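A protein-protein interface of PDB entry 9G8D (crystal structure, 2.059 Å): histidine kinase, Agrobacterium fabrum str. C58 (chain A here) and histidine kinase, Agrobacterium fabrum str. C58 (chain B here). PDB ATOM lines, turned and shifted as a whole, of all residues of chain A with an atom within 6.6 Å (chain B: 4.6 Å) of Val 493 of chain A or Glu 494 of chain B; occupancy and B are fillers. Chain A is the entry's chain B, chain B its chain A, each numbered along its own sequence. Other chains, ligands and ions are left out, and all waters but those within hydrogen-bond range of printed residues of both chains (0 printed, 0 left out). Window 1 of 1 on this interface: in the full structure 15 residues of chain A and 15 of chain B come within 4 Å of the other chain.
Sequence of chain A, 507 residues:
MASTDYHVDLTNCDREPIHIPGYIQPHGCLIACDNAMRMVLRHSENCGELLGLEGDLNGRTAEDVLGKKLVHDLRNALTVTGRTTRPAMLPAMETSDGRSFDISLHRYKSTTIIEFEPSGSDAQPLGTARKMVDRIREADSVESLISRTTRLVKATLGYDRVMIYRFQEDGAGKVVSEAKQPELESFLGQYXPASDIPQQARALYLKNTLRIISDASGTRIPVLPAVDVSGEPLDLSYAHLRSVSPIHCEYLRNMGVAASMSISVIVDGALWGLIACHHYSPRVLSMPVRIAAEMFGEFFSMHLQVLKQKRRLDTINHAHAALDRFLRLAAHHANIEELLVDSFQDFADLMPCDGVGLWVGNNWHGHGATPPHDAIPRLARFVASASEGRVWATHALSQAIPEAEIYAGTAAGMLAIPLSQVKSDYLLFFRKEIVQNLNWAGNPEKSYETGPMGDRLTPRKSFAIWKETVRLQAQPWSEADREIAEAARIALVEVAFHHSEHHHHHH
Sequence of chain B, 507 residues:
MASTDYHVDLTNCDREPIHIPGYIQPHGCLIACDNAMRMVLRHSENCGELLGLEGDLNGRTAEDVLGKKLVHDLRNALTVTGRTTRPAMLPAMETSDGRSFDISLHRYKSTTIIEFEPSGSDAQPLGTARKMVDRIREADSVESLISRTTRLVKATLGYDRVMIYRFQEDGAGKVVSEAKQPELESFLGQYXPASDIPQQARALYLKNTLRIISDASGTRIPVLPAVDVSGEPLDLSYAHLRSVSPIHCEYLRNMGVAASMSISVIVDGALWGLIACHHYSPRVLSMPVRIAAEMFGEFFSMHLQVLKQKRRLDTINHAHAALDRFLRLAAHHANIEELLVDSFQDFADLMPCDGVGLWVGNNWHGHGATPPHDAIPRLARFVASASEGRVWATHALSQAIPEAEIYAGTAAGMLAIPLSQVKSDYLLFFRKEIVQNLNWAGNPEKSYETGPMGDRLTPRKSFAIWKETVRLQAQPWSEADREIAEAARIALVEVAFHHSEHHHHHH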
ATOM      1  N   LEU A 327      26.225  26.502 -19.786  1.00  0.00           N
ATOM      2  CA  LEU A 327      26.186  25.474 -20.866  1.00  0.00           C
ATOM      3  C   LEU A 327      27.065  24.279 -20.474  1.00  0.00           C
ATOM      4  O   LEU A 327      26.589  23.146 -20.628  1.00  0.00           O
ATOM      5  CB  LEU A 327      26.630  26.086 -22.197  1.00  0.00           C
ATOM      6  CG  LEU A 327      25.534  26.820 -22.962  1.00  0.00           C
ATOM      7  CD1 LEU A 327      26.120  27.895 -23.876  1.00  0.00           C
ATOM      8  CD2 LEU A 327      24.692  25.843 -23.760  1.00  0.00           C
ATOM      9  N   GLY A 389       7.598  33.559 -30.126  1.00  0.00           N
ATOM     10  CA  GLY A 389       8.659  32.660 -29.633  1.00  0.00           C
ATOM     11  C   GLY A 389       9.993  33.368 -29.489  1.00  0.00           C
ATOM     12  O   GLY A 389      11.023  32.677 -29.496  1.00  0.00           O
ATOM     13  N   ARG A 390       9.993  34.699 -29.369  1.00  0.00           N
ATOM     14  CA  ARG A 390      11.225  35.476 -29.059  1.00  0.00           C
ATOM     15  C   ARG A 390      11.027  36.174 -27.707  1.00  0.00           C
ATOM     16  O   ARG A 390       9.962  35.998 -27.091  1.00  0.00           O
ATOM     17  CB  ARG A 390      11.538  36.477 -30.178  1.00  0.00           C
ATOM     18  CG  ARG A 390      12.963  36.404 -30.714  1.00  0.00           C
ATOM     19  CD  ARG A 390      13.082  35.494 -31.928  1.00  0.00           C
ATOM     20  NE  ARG A 390      14.382  35.563 -32.590  1.00  0.00           N
ATOM     21  CZ  ARG A 390      14.716  34.891 -33.694  1.00  0.00           C
ATOM     22  NH1 ARG A 390      13.848  34.081 -34.278  1.00  0.00           N
ATOM     23  NH2 ARG A 390      15.925  35.030 -34.210  1.00  0.00           N
ATOM     24  N   PRO A 418      11.226  32.907 -23.472  1.00  0.00           N
ATOM     25  CA  PRO A 418      10.593  31.608 -23.691  1.00  0.00           C
ATOM     26  C   PRO A 418      11.627  30.477 -23.611  1.00  0.00           C
ATOM     27  O   PRO A 418      12.724  30.635 -24.119  1.00  0.00           O
ATOM     28  CB  PRO A 418       9.964  31.735 -25.087  1.00  0.00           C
ATOM     29  CG  PRO A 418      10.818  32.773 -25.776  1.00  0.00           C
ATOM     30  CD  PRO A 418      11.235  33.741 -24.683  1.00  0.00           C
ATOM     31  N   LEU A 419      11.248  29.380 -22.949  1.00  0.00           N
ATOM     32  CA  LEU A 419      12.094  28.175 -22.748  1.00  0.00           C
ATOM     33  C   LEU A 419      11.670  27.052 -23.707  1.00  0.00           C
ATOM     34  O   LEU A 419      12.362  26.007 -23.729  1.00  0.00           O
ATOM     35  CB  LEU A 419      11.964  27.733 -21.291  1.00  0.00           C
ATOM     36  CG  LEU A 419      12.357  28.782 -20.252  1.00  0.00           C
ATOM     37  CD1 LEU A 419      12.203  28.236 -18.848  1.00  0.00           C
ATOM     38  CD2 LEU A 419      13.779  29.265 -20.473  1.00  0.00           C
ATOM     39  N   GLN A 421       9.003  26.311 -27.623  1.00  0.00           N
ATOM     40  CA  GLN A 421       8.040  26.751 -28.674  1.00  0.00           C
ATOM     41  C   GLN A 421       6.748  25.920 -28.610  1.00  0.00           C
ATOM     42  O   GLN A 421       5.813  26.258 -29.364  1.00  0.00           O
ATOM     43  CB  GLN A 421       8.664  26.670 -30.069  1.00  0.00           C
ATOM     44  CG  GLN A 421       9.574  27.846 -30.392  1.00  0.00           C
ATOM     45  CD  GLN A 421      10.028  27.853 -31.832  1.00  0.00           C
ATOM     46  OE1 GLN A 421       9.680  26.983 -32.629  1.00  0.00           O
ATOM     47  NE2 GLN A 421      10.830  28.845 -32.180  1.00  0.00           N
ATOM     48  N   GLU A 486      18.398  37.832 -25.294  1.00  0.00           N
ATOM     49  CA  GLU A 486      18.439  37.048 -26.552  1.00  0.00           C
ATOM     50  C   GLU A 486      19.570  36.018 -26.466  1.00  0.00           C
ATOM     51  O   GLU A 486      19.337  34.874 -26.875  1.00  0.00           O
ATOM     52  CB  GLU A 486      18.575  37.980 -27.758  1.00  0.00           C
ATOM     53  CG  GLU A 486      18.761  37.244 -29.076  1.00  0.00           C
ATOM     54  CD  GLU A 486      17.648  36.285 -29.462  1.00  0.00           C
ATOM     55  OE1 GLU A 486      16.555  36.361 -28.868  1.00  0.00           O
ATOM     56  OE2 GLU A 486      17.874  35.465 -30.370  1.00  0.00           O
ATOM     57  N   ALA A 488      20.696  34.759 -23.620  1.00  0.00           N
ATOM     58  CA  ALA A 488      20.144  33.816 -22.622  1.00  0.00           C
ATOM     59  C   ALA A 488      19.173  32.852 -23.321  1.00  0.00           C
ATOM     60  O   ALA A 488      19.300  31.626 -23.107  1.00  0.00           O
ATOM     61  CB  ALA A 488      19.501  34.569 -21.476  1.00  0.00           C
ATOM     62  N   ARG A 489      18.249  33.370 -24.134  1.00  0.00           N
ATOM     63  CA  ARG A 489      17.240  32.533 -24.850  1.00  0.00           C
ATOM     64  C   ARG A 489      17.973  31.461 -25.667  1.00  0.00           C
ATOM     65  O   ARG A 489      17.651  30.268 -25.547  1.00  0.00           O
ATOM     66  CB  ARG A 489      16.365  33.381 -25.778  1.00  0.00           C
ATOM     67  CG  ARG A 489      15.182  32.626 -26.379  1.00  0.00           C
ATOM     68  CD  ARG A 489      14.414  33.423 -27.418  1.00  0.00           C
ATOM     69  NE  ARG A 489      15.220  33.715 -28.597  1.00  0.00           N
ATOM     70  CZ  ARG A 489      15.508  32.847 -29.569  1.00  0.00           C
ATOM     71  NH1 ARG A 489      15.076  31.598 -29.516  1.00  0.00           N
ATOM     72  NH2 ARG A 489      16.258  33.224 -30.587  1.00  0.00           N
ATOM     73  N   ILE A 490      18.950  31.912 -26.447  1.00  0.00           N
ATOM     74  CA  ILE A 490      19.756  31.097 -27.404  1.00  0.00           C
ATOM     75  C   ILE A 490      20.591  30.058 -26.646  1.00  0.00           C
ATOM     76  O   ILE A 490      20.662  28.905 -27.099  1.00  0.00           O
ATOM     77  CB  ILE A 490      20.643  32.043 -28.233  1.00  0.00           C
ATOM     78  CG1 ILE A 490      19.818  32.887 -29.205  1.00  0.00           C
ATOM     79  CG2 ILE A 490      21.736  31.273 -28.940  1.00  0.00           C
ATOM     80  CD1 ILE A 490      19.267  32.117 -30.370  1.00  0.00           C
ATOM     81  N   ALA A 491      21.232  30.478 -25.553  1.00  0.00           N
ATOM     82  CA  ALA A 491      22.031  29.585 -24.683  1.00  0.00           C
ATOM     83  C   ALA A 491      21.129  28.459 -24.147  1.00  0.00           C
ATOM     84  O   ALA A 491      21.591  27.303 -24.077  1.00  0.00           O
ATOM     85  CB  ALA A 491      22.675  30.376 -23.570  1.00  0.00           C
ATOM     86  N   LEU A 492      19.878  28.779 -23.807  1.00  0.00           N
ATOM     87  CA  LEU A 492      18.922  27.827 -23.182  1.00  0.00           C
ATOM     88  C   LEU A 492      18.350  26.891 -24.257  1.00  0.00           C
ATOM     89  O   LEU A 492      18.147  25.709 -23.943  1.00  0.00           O
ATOM     90  CB  LEU A 492      17.822  28.604 -22.451  1.00  0.00           C
ATOM     91  CG  LEU A 492      18.238  29.190 -21.100  1.00  0.00           C
ATOM     92  CD1 LEU A 492      17.278  30.282 -20.653  1.00  0.00           C
ATOM     93  CD2 LEU A 492      18.331  28.111 -20.039  1.00  0.00           C
ATOM     94  N   VAL A 493      18.104  27.392 -25.472  1.00  0.00           N
ATOM     95  CA  VAL A 493      17.779  26.534 -26.654  1.00  0.00           C
ATOM     96  C   VAL A 493      18.899  25.501 -26.811  1.00  0.00           C
ATOM     97  O   VAL A 493      18.591  24.302 -27.001  1.00  0.00           O
ATOM     98  CB  VAL A 493      17.598  27.361 -27.939  1.00  0.00           C
ATOM     99  CG1 VAL A 493      17.750  26.506 -29.189  1.00  0.00           C
ATOM    100  CG2 VAL A 493      16.261  28.079 -27.943  1.00  0.00           C
ATOM    101  N   GLU A 494      20.149  25.953 -26.708  1.00  0.00           N
ATOM    102  CA  GLU A 494      21.347  25.108 -26.914  1.00  0.00           C
ATOM    103  C   GLU A 494      21.435  24.046 -25.804  1.00  0.00           C
ATOM    104  O   GLU A 494      21.791  22.885 -26.121  1.00  0.00           O
ATOM    105  CB  GLU A 494      22.599  25.972 -27.011  1.00  0.00           C
ATOM    106  CG  GLU A 494      23.786  25.154 -27.450  1.00  0.00           C
ATOM    107  CD  GLU A 494      25.010  25.891 -27.957  1.00  0.00           C
ATOM    108  OE1 GLU A 494      24.983  27.137 -28.049  1.00  0.00           O
ATOM    109  OE2 GLU A 494      26.001  25.192 -28.232  1.00  0.00           O
ATOM    110  N   VAL A 495      21.118  24.409 -24.557  1.00  0.00           N
ATOM    111  CA  VAL A 495      21.071  23.449 -23.412  1.00  0.00           C
ATOM    112  C   VAL A 495      20.020  22.374 -23.711  1.00  0.00           C
ATOM    113  O   VAL A 495      20.317  21.199 -23.489  1.00  0.00           O
ATOM    114  CB  VAL A 495      20.779  24.143 -22.068  1.00  0.00           C
ATOM    115  CG1 VAL A 495      20.401  23.140 -20.986  1.00  0.00           C
ATOM    116  CG2 VAL A 495      21.947  25.005 -21.615  1.00  0.00           C
ATOM    117  N   ALA A 496      18.824  22.770 -24.147  1.00  0.00           N
ATOM    118  CA  ALA A 496      17.704  21.837 -24.416  1.00  0.00           C
ATOM    119  C   ALA A 496      18.113  20.887 -25.557  1.00  0.00           C
ATOM    120  O   ALA A 496      17.954  19.653 -25.404  1.00  0.00           O
ATOM    121  CB  ALA A 496      16.447  22.610 -24.724  1.00  0.00           C
ATOM    122  N   PHE A 497      18.675  21.433 -26.641  1.00  0.00           N
ATOM    123  CA  PHE A 497      19.035  20.669 -27.864  1.00  0.00           C
ATOM    124  C   PHE A 497      20.096  19.613 -27.546  1.00  0.00           C
ATOM    125  O   PHE A 497      19.890  18.440 -27.906  1.00  0.00           O
ATOM    126  CB  PHE A 497      19.537  21.573 -28.993  1.00  0.00           C
ATOM    127  CG  PHE A 497      19.796  20.816 -30.273  1.00  0.00           C
ATOM    128  CD1 PHE A 497      18.748  20.226 -30.962  1.00  0.00           C
ATOM    129  CD2 PHE A 497      21.082  20.652 -30.762  1.00  0.00           C
ATOM    130  CE1 PHE A 497      18.979  19.509 -32.128  1.00  0.00           C
ATOM    131  CE2 PHE A 497      21.311  19.940 -31.930  1.00  0.00           C
ATOM    132  CZ  PHE A 497      20.260  19.371 -32.609  1.00  0.00           C
ATOM    133  N   HIS A 498      21.206  20.010 -26.918  1.00  0.00           N
ATOM    134  CA  HIS A 498      22.316  19.086 -26.572  1.00  0.00           C
ATOM    135  C   HIS A 498      21.793  18.032 -25.591  1.00  0.00           C
ATOM    136  O   HIS A 498      22.213  16.867 -25.706  1.00  0.00           O
ATOM    137  CB  HIS A 498      23.554  19.842 -26.071  1.00  0.00           C
ATOM    138  CG  HIS A 498      24.084  20.811 -27.073  1.00  0.00           C
ATOM    139  ND1 HIS A 498      24.030  20.570 -28.436  1.00  0.00           N
ATOM    140  CD2 HIS A 498      24.666  22.019 -26.923  1.00  0.00           C
ATOM    141  CE1 HIS A 498      24.548  21.595 -29.081  1.00  0.00           C
ATOM    142  NE2 HIS A 498      24.944  22.500 -28.173  1.00  0.00           N
ATOM    143  N   LEU B 327      16.479  31.279 -40.365  1.00  0.00           N
ATOM    144  CA  LEU B 327      15.670  30.714 -39.248  1.00  0.00           C
ATOM    145  C   LEU B 327      14.180  30.777 -39.602  1.00  0.00           C
ATOM    146  O   LEU B 327      13.482  29.761 -39.389  1.00  0.00           O
ATOM    147  CB  LEU B 327      15.960  31.483 -37.957  1.00  0.00           C
ATOM    148  CG  LEU B 327      17.042  30.884 -37.065  1.00  0.00           C
ATOM    149  CD1 LEU B 327      17.526  31.900 -36.035  1.00  0.00           C
ATOM    150  CD2 LEU B 327      16.536  29.630 -36.376  1.00  0.00           C
ATOM    151  N   ILE B 490      25.102  28.596 -33.865  1.00  0.00           N
ATOM    152  CA  ILE B 490      24.032  28.754 -32.844  1.00  0.00           C
ATOM    153  C   ILE B 490      22.672  28.894 -33.544  1.00  0.00           C
ATOM    154  O   ILE B 490      21.687  28.329 -33.027  1.00  0.00           O
ATOM    155  CB  ILE B 490      24.403  29.953 -31.958  1.00  0.00           C
ATOM    156  CG1 ILE B 490      25.275  29.528 -30.775  1.00  0.00           C
ATOM    157  CG2 ILE B 490      23.174  30.705 -31.532  1.00  0.00           C
ATOM    158  CD1 ILE B 490      26.016  30.678 -30.129  1.00  0.00           C
ATOM    159  N   ALA B 491      22.613  29.619 -34.669  1.00  0.00           N
ATOM    160  CA  ALA B 491      21.418  29.697 -35.541  1.00  0.00           C
ATOM    161  C   ALA B 491      21.029  28.291 -36.021  1.00  0.00           C
ATOM    162  O   ALA B 491      19.824  27.973 -36.016  1.00  0.00           O
ATOM    163  CB  ALA B 491      21.657  30.613 -36.709  1.00  0.00           C
ATOM    164  N   LEU B 492      22.007  27.483 -36.436  1.00  0.00           N
ATOM    165  CA  LEU B 492      21.757  26.120 -36.967  1.00  0.00           C
ATOM    166  C   LEU B 492      21.306  25.188 -35.835  1.00  0.00           C
ATOM    167  O   LEU B 492      20.404  24.368 -36.095  1.00  0.00           O
ATOM    168  CB  LEU B 492      23.008  25.620 -37.693  1.00  0.00           C
ATOM    169  CG  LEU B 492      23.327  26.373 -38.990  1.00  0.00           C
ATOM    170  CD1 LEU B 492      24.757  26.134 -39.432  1.00  0.00           C
ATOM    171  CD2 LEU B 492      22.366  25.991 -40.105  1.00  0.00           C
ATOM    172  N   VAL B 493      21.859  25.324 -34.623  1.00  0.00           N
ATOM    173  CA  VAL B 493      21.386  24.562 -33.425  1.00  0.00           C
ATOM    174  C   VAL B 493      19.894  24.842 -33.241  1.00  0.00           C
ATOM    175  O   VAL B 493      19.116  23.886 -33.023  1.00  0.00           O
ATOM    176  CB  VAL B 493      22.160  24.930 -32.148  1.00  0.00           C
ATOM    177  CG1 VAL B 493      21.376  24.571 -30.891  1.00  0.00           C
ATOM    178  CG2 VAL B 493      23.534  24.285 -32.128  1.00  0.00           C
ATOM    179  N   GLU B 494      19.524  26.121 -33.329  1.00  0.00           N
ATOM    180  CA  GLU B 494      18.134  26.600 -33.138  1.00  0.00           C
ATOM    181  C   GLU B 494      17.227  26.015 -34.234  1.00  0.00           C
ATOM    182  O   GLU B 494      16.132  25.514 -33.878  1.00  0.00           O
ATOM    183  CB  GLU B 494      18.115  28.123 -33.078  1.00  0.00           C
ATOM    184  CG  GLU B 494      16.732  28.650 -32.787  1.00  0.00           C
ATOM    185  CD  GLU B 494      16.642  30.065 -32.252  1.00  0.00           C
ATOM    186  OE1 GLU B 494      17.680  30.759 -32.183  1.00  0.00           O
ATOM    187  OE2 GLU B 494      15.512  30.469 -31.928  1.00  0.00           O
ATOM    188  N   VAL B 495      17.659  26.040 -35.500  1.00  0.00           N
ATOM    189  CA  VAL B 495      16.918  25.395 -36.629  1.00  0.00           C
ATOM    190  C   VAL B 495      16.639  23.938 -36.249  1.00  0.00           C
ATOM    191  O   VAL B 495      15.472  23.532 -36.323  1.00  0.00           O
ATOM    192  CB  VAL B 495      17.677  25.483 -37.969  1.00  0.00           C
ATOM    193  CG1 VAL B 495      17.110  24.518 -39.001  1.00  0.00           C
ATOM    194  CG2 VAL B 495      17.691  26.902 -38.511  1.00  0.00           C
ATOM    195  N   ALA B 496      17.665  23.194 -35.836  1.00  0.00           N
ATOM    196  CA  ALA B 496      17.569  21.748 -35.523  1.00  0.00           C
ATOM    197  C   ALA B 496      16.627  21.535 -34.329  1.00  0.00           C
ATOM    198  O   ALA B 496      15.771  20.629 -34.404  1.00  0.00           O
ATOM    199  CB  ALA B 496      18.937  21.169 -35.266  1.00  0.00           C
ATOM    200  N   PHE B 497      16.760  22.347 -33.276  1.00  0.00           N
ATOM    201  CA  PHE B 497      15.934  22.236 -32.046  1.00  0.00           C
ATOM    202  C   PHE B 497      14.459  22.485 -32.380  1.00  0.00           C
ATOM    203  O   PHE B 497      13.622  21.637 -31.999  1.00  0.00           O
ATOM    204  CB  PHE B 497      16.394  23.197 -30.950  1.00  0.00           C
ATOM    205  CG  PHE B 497      15.560  23.095 -29.697  1.00  0.00           C
ATOM    206  CD1 PHE B 497      15.531  21.918 -28.964  1.00  0.00           C
ATOM    207  CD2 PHE B 497      14.786  24.160 -29.266  1.00  0.00           C
ATOM    208  CE1 PHE B 497      14.760  21.817 -27.816  1.00  0.00           C
ATOM    209  CE2 PHE B 497      14.017  24.057 -28.117  1.00  0.00           C
ATOM    210  CZ  PHE B 497      14.002  22.884 -27.397  1.00  0.00           C
ATOM    211  N   HIS B 498      14.141  23.603 -33.039  1.00  0.00           N
ATOM    212  CA  HIS B 498      12.739  23.987 -33.368  1.00  0.00           C
ATOM    213  C   HIS B 498      12.136  22.924 -34.289  1.00  0.00           C
ATOM    214  O   HIS B 498      10.924  22.677 -34.190  1.00  0.00           O
ATOM    215  CB  HIS B 498      12.639  25.394 -33.968  1.00  0.00           C
ATOM    216  CG  HIS B 498      13.084  26.474 -33.042  1.00  0.00           C
ATOM    217  ND1 HIS B 498      12.902  26.398 -31.672  1.00  0.00           N
ATOM    218  CD2 HIS B 498      13.695  27.653 -33.280  1.00  0.00           C
ATOM    219  CE1 HIS B 498      13.391  27.482 -31.105  1.00  0.00           C
ATOM    220  NE2 HIS B 498      13.883  28.269 -32.072  1.00  0.00           N
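Among the printed residues, pairs that only touch across the chains: Arg 390 of chain A with Leu 327 of chain B, Ile 490 of chain A with Ile 490 of chain B, Ile 490 of chain A with Glu 494 of chain B, Val 493 of chain A with Glu 494 of chain B, Val 493 of chain A with Phe 497 of chain B, Glu 494 of chain A with Ile 490 of chain B, Ala 496 of chain A with Phe 497 of chain B, Phe 497 of chain A with Val 493 of chain B, Phe 497 of chain A with Ala 496 of chain B and Phe 497 of chain A with Phe 497 of chain B.
The guanidinium group of Arg 489 of chain A is in salt-bridge range of the side-chain carboxylate of Glu 494 of chain B (2.7 Å). A ring nitrogen (NE2) of His 498 of chain B sits close to the side-chain amide nitrogen of Gln 421 of chain A (3.1 Å).
OE2 of Glu 486 of chain A is in salt-bridge range of NH2 of Arg 489 of chain A (2.8 Å). The side-chain carboxylate (OE2) of Glu 494 of chain A lies within hydrogen-bond range of a ring nitrogen (NE2) of His 498 of chain A (2.9 Å). NE2 of His 498 of chain B is in hydrogen-bond range of OE2 of Glu 494 of chain B, 2.7 Å away.
Of the 18 printed residues of chain A, 8 touch a printed residue of chain B. Of the 10 printed residues of chain B, 7 touch a printed residue of chain A. Among the printed residues, 12 pairs touch across the chains. Among the printed residues, Asp or Glu carboxylates within 4 Å of a Lys or Arg side-chain nitrogen of the other chain: Arg 489 of chain A with Glu 494 of chain B (2.7 Å).
Glu 486 of chain A touches none of the printed residues of chain B. Printed residues of chain B within 4 Å of Arg 489 of chain A: Glu 494 (2.7 Å). Val 493 of chain A touches just these residues of chain B: Glu 494 (3.97 Å) and Phe 497 (3.8 Å). Of the printed residues of chain B, Ala 496 of chain A touches Phe 497. Printed residues of chain B within 4 Å of Phe 497 of chain A: Val 493, Ala 496 and Phe 497. Of the printed residues of chain A, Glu 494 of chain B touches Arg 489 (2.7 Å), Ile 490 (2.8 Å) and Val 493 (3.97 Å). Val 495 of chain B touches none of the printed residues of chain A. Printed residues of chain A within 4 Å of Phe 497 of chain B: Val 493 (3.8 Å), Ala 496 (3.6 Å) and Phe 497 (3.6 Å). Of the printed residues of chain A, His 498 of chain B touches Gln 421. The nearest residue of chain B that does not touch Val 493 of chain A is His 498 of chain B (4.3 Å). The nearest printed residue of chain B that does not touch Gln 421 of chain A is Glu 494 of chain B (5.0 Å).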
